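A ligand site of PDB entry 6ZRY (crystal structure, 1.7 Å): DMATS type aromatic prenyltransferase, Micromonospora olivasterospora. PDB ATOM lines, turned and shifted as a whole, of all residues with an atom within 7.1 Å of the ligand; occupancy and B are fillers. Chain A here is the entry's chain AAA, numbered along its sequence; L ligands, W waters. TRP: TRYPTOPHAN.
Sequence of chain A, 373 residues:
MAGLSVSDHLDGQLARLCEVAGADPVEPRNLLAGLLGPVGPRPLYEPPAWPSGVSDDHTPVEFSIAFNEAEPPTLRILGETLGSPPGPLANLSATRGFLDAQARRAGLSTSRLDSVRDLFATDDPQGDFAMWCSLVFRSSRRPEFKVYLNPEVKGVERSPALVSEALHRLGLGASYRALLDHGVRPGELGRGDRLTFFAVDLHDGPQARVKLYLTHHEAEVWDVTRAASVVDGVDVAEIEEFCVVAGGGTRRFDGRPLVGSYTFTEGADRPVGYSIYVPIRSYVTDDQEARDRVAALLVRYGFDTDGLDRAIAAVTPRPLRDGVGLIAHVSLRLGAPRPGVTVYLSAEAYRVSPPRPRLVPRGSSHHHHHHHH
The guanidinium group (NH2) of Arg 281 lies within salt-bridge range of an oxygen (OXT) of the ligand (3.0 Å). OE2 of Glu 62 is in hydrogen-bond range of NE1 of the ligand. The backbone carbonyl oxygen (O) of Gly 53 is in hydrogen-bond range of a nitrogen (N) of the ligand (3.1 Å). An oxygen (OXT) of the ligand sits close to a ring nitrogen (NE2) of His 329, 3.3 Å away. The backbone carbonyl oxygen of Val 54 lies within hydrogen-bond range of a nitrogen (N) of the ligand, 3.0 Å away.
The backbone carbonyl oxygen (O) of Phe 197 is in hydrogen-bond range of the backbone NH (N) of Tyr 213. A ring nitrogen (NE2) of His 329 sits at hydrogen-bond distance from the guanidinium group (NH1) of Arg 281, at 3.3 Å. NE of Arg 281 lies within salt-bridge range of OD2 of Asp 56, at 2.7 Å. The guanidinium group of Arg 281 sits at hydrogen-bond distance from the backbone carbonyl oxygen of Ala 328 (2.9 Å). The backbone NH (N) of Glu 62 is in hydrogen-bond range of the backbone carbonyl oxygen (O) of Leu 78 (2.8 Å). N of Tyr 344 is in hydrogen-bond range of O of His 329. N of Val 54 lies close to OG of Ser 52 (3.2 Å).
Residues that only touch the ligand: Phe 197 and Ser 55. Hydrophobic or aromatic side chains within 4 Å of the ligand: Phe 197 and His 329. Within 4 Å of the ligand: Gly 53, Val 54, Ser 55, Glu 62, Phe 197, Arg 281 and His 329.
Water W1 bridges a nitrogen (N) of the ligand and the side-chain carboxylate (OD1) of Asp 56. Water W2 bridges an oxygen (OXT) of the ligand (2.7 Å) and the guanidinium group (NH2) of Arg 281 (3.2 Å). Water W4 lies within hydrogen-bond range of OE1 of Glu 62 (2.7 Å), N of the ligand (2.8 Å) and NE2 of His 329 (2.9 Å).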
ATOM      1  N   SER A  52     -24.110  -2.319 -18.593  1.00  0.00           N
ATOM      2  CA  SER A  52     -24.766  -3.642 -18.728  1.00  0.00           C
ATOM      3  C   SER A  52     -24.206  -4.387 -19.948  1.00  0.00           C
ATOM      4  O   SER A  52     -24.053  -3.781 -20.997  1.00  0.00           O
ATOM      5  CB  SER A  52     -26.256  -3.488 -18.811  1.00  0.00           C
ATOM      6  OG  SER A  52     -26.916  -4.681 -19.152  1.00  0.00           O
ATOM      7  N   GLY A  53     -23.905  -5.675 -19.798  1.00  0.00           N
ATOM      8  CA  GLY A  53     -23.463  -6.489 -20.925  1.00  0.00           C
ATOM      9  C   GLY A  53     -24.606  -6.952 -21.824  1.00  0.00           C
ATOM     10  O   GLY A  53     -24.287  -7.593 -22.843  1.00  0.00           O
ATOM     11  N   VAL A  54     -25.874  -6.638 -21.499  1.00  0.00           N
ATOM     12  CA  VAL A  54     -27.058  -7.138 -22.254  1.00  0.00           C
ATOM     13  C   VAL A  54     -26.952  -6.663 -23.735  1.00  0.00           C
ATOM     14  O   VAL A  54     -27.309  -7.436 -24.629  1.00  0.00           O
ATOM     15  CB  VAL A  54     -28.389  -6.695 -21.630  1.00  0.00           C
ATOM     16  CG1 VAL A  54     -29.599  -7.046 -22.506  1.00  0.00           C
ATOM     17  CG2 VAL A  54     -28.581  -7.324 -20.259  1.00  0.00           C
ATOM     18  N   SER A  55     -26.455  -5.452 -23.966  1.00  0.00           N
ATOM     19  CA  SER A  55     -26.361  -4.854 -25.317  1.00  0.00           C
ATOM     20  C   SER A  55     -25.107  -3.969 -25.395  1.00  0.00           C
ATOM     21  O   SER A  55     -24.575  -3.597 -24.349  1.00  0.00           O
ATOM     22  CB  SER A  55     -27.587  -4.075 -25.675  1.00  0.00           C
ATOM     23  OG  SER A  55     -27.685  -2.866 -24.867  1.00  0.00           O
ATOM     24  N   ASP A  56     -24.644  -3.708 -26.625  1.00  0.00           N
ATOM     25  CA  ASP A  56     -23.392  -2.974 -26.912  1.00  0.00           C
ATOM     26  C   ASP A  56     -23.485  -1.550 -26.347  1.00  0.00           C
ATOM     27  O   ASP A  56     -22.437  -1.056 -25.890  1.00  0.00           O
ATOM     28  CB  ASP A  56     -23.093  -2.917 -28.414  1.00  0.00           C
ATOM     29  CG  ASP A  56     -22.598  -4.225 -29.021  1.00  0.00           C
ATOM     30  OD1 ASP A  56     -22.444  -5.230 -28.287  1.00  0.00           O
ATOM     31  OD2 ASP A  56     -22.396  -4.258 -30.236  1.00  0.00           O
ATOM     32  N   GLU A  62     -32.695  -6.437 -24.459  1.00  0.00           N
ATOM     33  CA  GLU A  62     -32.572  -6.765 -25.907  1.00  0.00           C
ATOM     34  C   GLU A  62     -33.833  -7.515 -26.307  1.00  0.00           C
ATOM     35  O   GLU A  62     -34.277  -8.389 -25.550  1.00  0.00           O
ATOM     36  CB  GLU A  62     -31.345  -7.621 -26.171  1.00  0.00           C
ATOM     37  CG  GLU A  62     -31.185  -7.986 -27.631  1.00  0.00           C
ATOM     38  CD  GLU A  62     -29.946  -8.802 -27.937  1.00  0.00           C
ATOM     39  OE1 GLU A  62     -28.902  -8.213 -28.278  1.00  0.00           O
ATOM     40  OE2 GLU A  62     -30.036 -10.028 -27.790  1.00  0.00           O
ATOM     41  N   LEU A  78     -34.648 -10.111 -23.255  1.00  0.00           N
ATOM     42  CA  LEU A  78     -33.554 -10.479 -22.341  1.00  0.00           C
ATOM     43  C   LEU A  78     -33.145  -9.232 -21.591  1.00  0.00           C
ATOM     44  O   LEU A  78     -32.946  -8.203 -22.241  1.00  0.00           O
ATOM     45  CB  LEU A  78     -32.395 -11.049 -23.157  1.00  0.00           C
ATOM     46  CG  LEU A  78     -31.162 -11.480 -22.363  1.00  0.00           C
ATOM     47  CD1 LEU A  78     -31.447 -12.747 -21.568  1.00  0.00           C
ATOM     48  CD2 LEU A  78     -29.995 -11.713 -23.277  1.00  0.00           C
ATOM     49  N   TRP A 132     -29.459 -12.960 -15.366  1.00  0.00           N
ATOM     50  CA  TRP A 132     -30.328 -12.222 -16.296  1.00  0.00           C
ATOM     51  C   TRP A 132     -31.669 -12.937 -16.370  1.00  0.00           C
ATOM     52  O   TRP A 132     -31.786 -14.067 -15.927  1.00  0.00           O
ATOM     53  CB  TRP A 132     -29.685 -12.087 -17.680  1.00  0.00           C
ATOM     54  CG  TRP A 132     -28.554 -11.105 -17.775  1.00  0.00           C
ATOM     55  CD1 TRP A 132     -28.087 -10.259 -16.803  1.00  0.00           C
ATOM     56  CD2 TRP A 132     -27.686 -10.935 -18.892  1.00  0.00           C
ATOM     57  NE1 TRP A 132     -27.025  -9.539 -17.281  1.00  0.00           N
ATOM     58  CE2 TRP A 132     -26.733  -9.956 -18.542  1.00  0.00           C
ATOM     59  CE3 TRP A 132     -27.619 -11.513 -20.162  1.00  0.00           C
ATOM     60  CZ2 TRP A 132     -25.752  -9.521 -19.418  1.00  0.00           C
ATOM     61  CZ3 TRP A 132     -26.636 -11.108 -21.029  1.00  0.00           C
ATOM     62  CH2 TRP A 132     -25.700 -10.130 -20.661  1.00  0.00           C
ATOM     63  N   THR A 196     -20.984 -19.661 -20.895  1.00  0.00           N
ATOM     64  CA  THR A 196     -21.451 -18.255 -20.907  1.00  0.00           C
ATOM     65  C   THR A 196     -22.787 -18.128 -20.180  1.00  0.00           C
ATOM     66  O   THR A 196     -22.955 -17.156 -19.451  1.00  0.00           O
ATOM     67  CB  THR A 196     -21.519 -17.713 -22.331  1.00  0.00           C
ATOM     68  OG1 THR A 196     -20.198 -17.840 -22.868  1.00  0.00           O
ATOM     69  CG2 THR A 196     -21.985 -16.280 -22.362  1.00  0.00           C
ATOM     70  N   PHE A 197     -23.744 -19.008 -20.445  1.00  0.00           N
ATOM     71  CA  PHE A 197     -25.054 -18.977 -19.766  1.00  0.00           C
ATOM     72  C   PHE A 197     -25.469 -20.379 -19.345  1.00  0.00           C
ATOM     73  O   PHE A 197     -25.302 -21.319 -20.117  1.00  0.00           O
ATOM     74  CB  PHE A 197     -26.195 -18.462 -20.664  1.00  0.00           C
ATOM     75  CG  PHE A 197     -26.019 -17.053 -21.208  1.00  0.00           C
ATOM     76  CD1 PHE A 197     -25.912 -15.969 -20.355  1.00  0.00           C
ATOM     77  CD2 PHE A 197     -26.014 -16.830 -22.574  1.00  0.00           C
ATOM     78  CE1 PHE A 197     -25.806 -14.681 -20.864  1.00  0.00           C
ATOM     79  CE2 PHE A 197     -25.898 -15.544 -23.080  1.00  0.00           C
ATOM     80  CZ  PHE A 197     -25.785 -14.472 -22.222  1.00  0.00           C
ATOM     81  N   TYR A 213     -25.021 -22.435 -22.832  1.00  0.00           N
ATOM     82  CA  TYR A 213     -24.455 -21.674 -23.967  1.00  0.00           C
ATOM     83  C   TYR A 213     -22.935 -21.634 -23.844  1.00  0.00           C
ATOM     84  O   TYR A 213     -22.451 -21.295 -22.733  1.00  0.00           O
ATOM     85  CB  TYR A 213     -24.975 -20.248 -23.965  1.00  0.00           C
ATOM     86  CG  TYR A 213     -26.428 -20.031 -24.265  1.00  0.00           C
ATOM     87  CD1 TYR A 213     -27.428 -20.503 -23.424  1.00  0.00           C
ATOM     88  CD2 TYR A 213     -26.825 -19.221 -25.325  1.00  0.00           C
ATOM     89  CE1 TYR A 213     -28.772 -20.250 -23.667  1.00  0.00           C
ATOM     90  CE2 TYR A 213     -28.164 -18.950 -25.573  1.00  0.00           C
ATOM     91  CZ  TYR A 213     -29.142 -19.471 -24.733  1.00  0.00           C
ATOM     92  OH  TYR A 213     -30.467 -19.212 -24.931  1.00  0.00           O
ATOM     93  N   THR A 215     -19.426 -19.995 -25.665  1.00  0.00           N
ATOM     94  CA  THR A 215     -18.863 -18.980 -26.571  1.00  0.00           C
ATOM     95  C   THR A 215     -17.578 -19.544 -27.133  1.00  0.00           C
ATOM     96  O   THR A 215     -16.701 -19.942 -26.335  1.00  0.00           O
ATOM     97  CB  THR A 215     -18.667 -17.637 -25.859  1.00  0.00           C
ATOM     98  OG1 THR A 215     -19.946 -17.219 -25.354  1.00  0.00           O
ATOM     99  CG2 THR A 215     -18.094 -16.584 -26.774  1.00  0.00           C
ATOM    100  N   ARG A 256     -16.768 -10.716 -33.356  1.00  0.00           N
ATOM    101  CA  ARG A 256     -17.572 -11.216 -32.234  1.00  0.00           C
ATOM    102  C   ARG A 256     -17.755 -12.720 -32.437  1.00  0.00           C
ATOM    103  O   ARG A 256     -17.872 -13.176 -33.575  1.00  0.00           O
ATOM    104  CB  ARG A 256     -18.870 -10.440 -32.111  1.00  0.00           C
ATOM    105  CG  ARG A 256     -18.650  -9.008 -31.692  1.00  0.00           C
ATOM    106  CD  ARG A 256     -19.958  -8.323 -31.391  1.00  0.00           C
ATOM    107  NE  ARG A 256     -19.809  -6.884 -31.228  1.00  0.00           N
ATOM    108  CZ  ARG A 256     -19.481  -6.256 -30.098  1.00  0.00           C
ATOM    109  NH1 ARG A 256     -19.240  -6.932 -28.989  1.00  0.00           N
ATOM    110  NH2 ARG A 256     -19.386  -4.938 -30.091  1.00  0.00           N
ATOM    111  N   PRO A 257     -17.694 -13.507 -31.343  1.00  0.00           N
ATOM    112  CA  PRO A 257     -17.596 -14.964 -31.454  1.00  0.00           C
ATOM    113  C   PRO A 257     -18.942 -15.631 -31.761  1.00  0.00           C
ATOM    114  O   PRO A 257     -19.957 -15.157 -31.311  1.00  0.00           O
ATOM    115  CB  PRO A 257     -17.110 -15.378 -30.051  1.00  0.00           C
ATOM    116  CG  PRO A 257     -17.672 -14.336 -29.134  1.00  0.00           C
ATOM    117  CD  PRO A 257     -17.644 -13.051 -29.951  1.00  0.00           C
ATOM    118  N   VAL A 259     -21.624 -18.474 -30.967  1.00  0.00           N
ATOM    119  CA  VAL A 259     -22.122 -19.038 -29.700  1.00  0.00           C
ATOM    120  C   VAL A 259     -22.999 -20.213 -30.054  1.00  0.00           C
ATOM    121  O   VAL A 259     -23.809 -20.127 -30.981  1.00  0.00           O
ATOM    122  CB  VAL A 259     -22.855 -17.995 -28.855  1.00  0.00           C
ATOM    123  CG1 VAL A 259     -23.498 -18.604 -27.638  1.00  0.00           C
ATOM    124  CG2 VAL A 259     -21.929 -16.878 -28.460  1.00  0.00           C
ATOM    125  N   TYR A 277     -25.716 -19.144 -32.782  1.00  0.00           N
ATOM    126  CA  TYR A 277     -25.991 -17.693 -32.689  1.00  0.00           C
ATOM    127  C   TYR A 277     -24.856 -16.974 -33.375  1.00  0.00           C
ATOM    128  O   TYR A 277     -23.728 -17.014 -32.897  1.00  0.00           O
ATOM    129  CB  TYR A 277     -26.159 -17.232 -31.241  1.00  0.00           C
ATOM    130  CG  TYR A 277     -27.139 -18.026 -30.419  1.00  0.00           C
ATOM    131  CD1 TYR A 277     -26.776 -19.259 -29.905  1.00  0.00           C
ATOM    132  CD2 TYR A 277     -28.406 -17.561 -30.132  1.00  0.00           C
ATOM    133  CE1 TYR A 277     -27.659 -20.031 -29.175  1.00  0.00           C
ATOM    134  CE2 TYR A 277     -29.299 -18.303 -29.382  1.00  0.00           C
ATOM    135  CZ  TYR A 277     -28.918 -19.551 -28.903  1.00  0.00           C
ATOM    136  OH  TYR A 277     -29.781 -20.302 -28.153  1.00  0.00           O
ATOM    137  N   VAL A 278     -25.142 -16.371 -34.525  1.00  0.00           N
ATOM    138  CA  VAL A 278     -24.168 -15.560 -35.247  1.00  0.00           C
ATOM    139  C   VAL A 278     -24.358 -14.104 -34.834  1.00  0.00           C
ATOM    140  O   VAL A 278     -25.440 -13.532 -35.079  1.00  0.00           O
ATOM    141  CB  VAL A 278     -24.298 -15.724 -36.765  1.00  0.00           C
ATOM    142  CG1 VAL A 278     -23.307 -14.869 -37.508  1.00  0.00           C
ATOM    143  CG2 VAL A 278     -24.174 -17.192 -37.179  1.00  0.00           C
ATOM    144  N   PRO A 279     -23.299 -13.437 -34.324  1.00  0.00           N
ATOM    145  CA  PRO A 279     -23.353 -11.996 -34.015  1.00  0.00           C
ATOM    146  C   PRO A 279     -23.130 -11.204 -35.303  1.00  0.00           C
ATOM    147  O   PRO A 279     -22.054 -10.579 -35.508  1.00  0.00           O
ATOM    148  CB  PRO A 279     -22.244 -11.857 -32.995  1.00  0.00           C
ATOM    149  CG  PRO A 279     -21.197 -12.839 -33.496  1.00  0.00           C
ATOM    150  CD  PRO A 279     -21.986 -14.015 -34.002  1.00  0.00           C
ATOM    151  N   ARG A 281     -23.982  -8.461 -36.525  1.00  0.00           N
ATOM    152  CA  ARG A 281     -23.574  -7.033 -36.482  1.00  0.00           C
ATOM    153  C   ARG A 281     -22.071  -6.891 -36.688  1.00  0.00           C
ATOM    154  O   ARG A 281     -21.624  -5.805 -37.127  1.00  0.00           O
ATOM    155  CB  ARG A 281     -23.956  -6.386 -35.145  1.00  0.00           C
ATOM    156  CG  ARG A 281     -23.208  -6.937 -33.927  1.00  0.00           C
ATOM    157  CD  ARG A 281     -23.823  -6.295 -32.707  1.00  0.00           C
ATOM    158  NE  ARG A 281     -23.236  -6.566 -31.425  1.00  0.00           N
ATOM    159  CZ  ARG A 281     -23.322  -7.705 -30.735  1.00  0.00           C
ATOM    160  NH1 ARG A 281     -23.910  -8.777 -31.228  1.00  0.00           N
ATOM    161  NH2 ARG A 281     -22.795  -7.763 -29.526  1.00  0.00           N
ATOM    162  N   ALA A 328     -28.602  -7.561 -33.923  1.00  0.00           N
ATOM    163  CA  ALA A 328     -27.436  -7.839 -33.076  1.00  0.00           C
ATOM    164  C   ALA A 328     -26.924  -9.263 -33.329  1.00  0.00           C
ATOM    165  O   ALA A 328     -25.692  -9.494 -33.334  1.00  0.00           O
ATOM    166  CB  ALA A 328     -27.827  -7.667 -31.628  1.00  0.00           C
ATOM    167  N   HIS A 329     -27.842 -10.188 -33.473  1.00  0.00           N
ATOM    168  CA  HIS A 329     -27.609 -11.631 -33.664  1.00  0.00           C
ATOM    169  C   HIS A 329     -28.675 -12.209 -34.583  1.00  0.00           C
ATOM    170  O   HIS A 329     -29.793 -11.640 -34.674  1.00  0.00           O
ATOM    171  CB  HIS A 329     -27.634 -12.400 -32.349  1.00  0.00           C
ATOM    172  CG  HIS A 329     -26.788 -11.863 -31.263  1.00  0.00           C
ATOM    173  ND1 HIS A 329     -25.543 -12.364 -31.014  1.00  0.00           N
ATOM    174  CD2 HIS A 329     -27.016 -10.928 -30.331  1.00  0.00           C
ATOM    175  CE1 HIS A 329     -25.024 -11.736 -29.948  1.00  0.00           C
ATOM    176  NE2 HIS A 329     -25.904 -10.837 -29.532  1.00  0.00           N
ATOM    177  N   SER A 331     -30.035 -16.442 -35.170  1.00  0.00           N
ATOM    178  CA  SER A 331     -29.817 -17.805 -34.659  1.00  0.00           C
ATOM    179  C   SER A 331     -30.677 -18.806 -35.400  1.00  0.00           C
ATOM    180  O   SER A 331     -31.772 -18.492 -35.822  1.00  0.00           O
ATOM    181  CB  SER A 331     -30.015 -17.879 -33.149  1.00  0.00           C
ATOM    182  OG  SER A 331     -31.413 -17.901 -32.818  1.00  0.00           O
ATOM    183  N   TYR A 344     -32.448 -10.954 -33.315  1.00  0.00           N
ATOM    184  CA  TYR A 344     -32.227 -10.236 -32.045  1.00  0.00           C
ATOM    185  C   TYR A 344     -32.121  -8.763 -32.421  1.00  0.00           C
ATOM    186  O   TYR A 344     -31.254  -8.426 -33.270  1.00  0.00           O
ATOM    187  CB  TYR A 344     -31.032 -10.820 -31.306  1.00  0.00           C
ATOM    188  CG  TYR A 344     -31.190 -12.275 -30.959  1.00  0.00           C
ATOM    189  CD1 TYR A 344     -31.042 -13.240 -31.932  1.00  0.00           C
ATOM    190  CD2 TYR A 344     -31.490 -12.688 -29.674  1.00  0.00           C
ATOM    191  CE1 TYR A 344     -31.189 -14.586 -31.651  1.00  0.00           C
ATOM    192  CE2 TYR A 344     -31.665 -14.043 -29.374  1.00  0.00           C
ATOM    193  CZ  TYR A 344     -31.474 -14.983 -30.367  1.00  0.00           C
ATOM    194  OH  TYR A 344     -31.641 -16.318 -30.148  1.00  0.00           O
HETATM  195  N   TRP L   1     -24.710  -8.483 -25.785  1.00  0.00           N
HETATM  196  CA  TRP L   1     -24.033  -9.729 -25.292  1.00  0.00           C
HETATM  197  C   TRP L   1     -23.232 -10.372 -26.425  1.00  0.00           C
HETATM  198  O   TRP L   1     -22.418 -11.269 -26.167  1.00  0.00           O
HETATM  199  CB  TRP L   1     -25.045 -10.720 -24.681  1.00  0.00           C
HETATM  200  CG  TRP L   1     -26.068 -11.242 -25.630  1.00  0.00           C
HETATM  201  CD1 TRP L   1     -27.244 -10.644 -26.002  1.00  0.00           C
HETATM  202  CD2 TRP L   1     -26.029 -12.496 -26.349  1.00  0.00           C
HETATM  203  NE1 TRP L   1     -27.922 -11.429 -26.903  1.00  0.00           N
HETATM  204  CE2 TRP L   1     -27.214 -12.578 -27.114  1.00  0.00           C
HETATM  205  CE3 TRP L   1     -25.119 -13.564 -26.390  1.00  0.00           C
HETATM  206  CZ2 TRP L   1     -27.491 -13.669 -27.939  1.00  0.00           C
HETATM  207  CZ3 TRP L   1     -25.398 -14.639 -27.199  1.00  0.00           C
HETATM  208  CH2 TRP L   1     -26.567 -14.692 -27.959  1.00  0.00           C
HETATM  209  OXT TRP L   1     -23.397  -9.986 -27.605  1.00  0.00           O
HETATM  210  O   HOH W   1     -22.949  -6.509 -25.933  1.00  0.00           O
HETATM  211  O   HOH W   2     -21.651 -10.717 -29.558  1.00  0.00           O
HETATM  212  O   HOH W   3     -21.088 -13.108 -27.236  1.00  0.00           O
HETATM  213  O   HOH W   4     -26.252  -8.286 -28.158  1.00  0.00           O
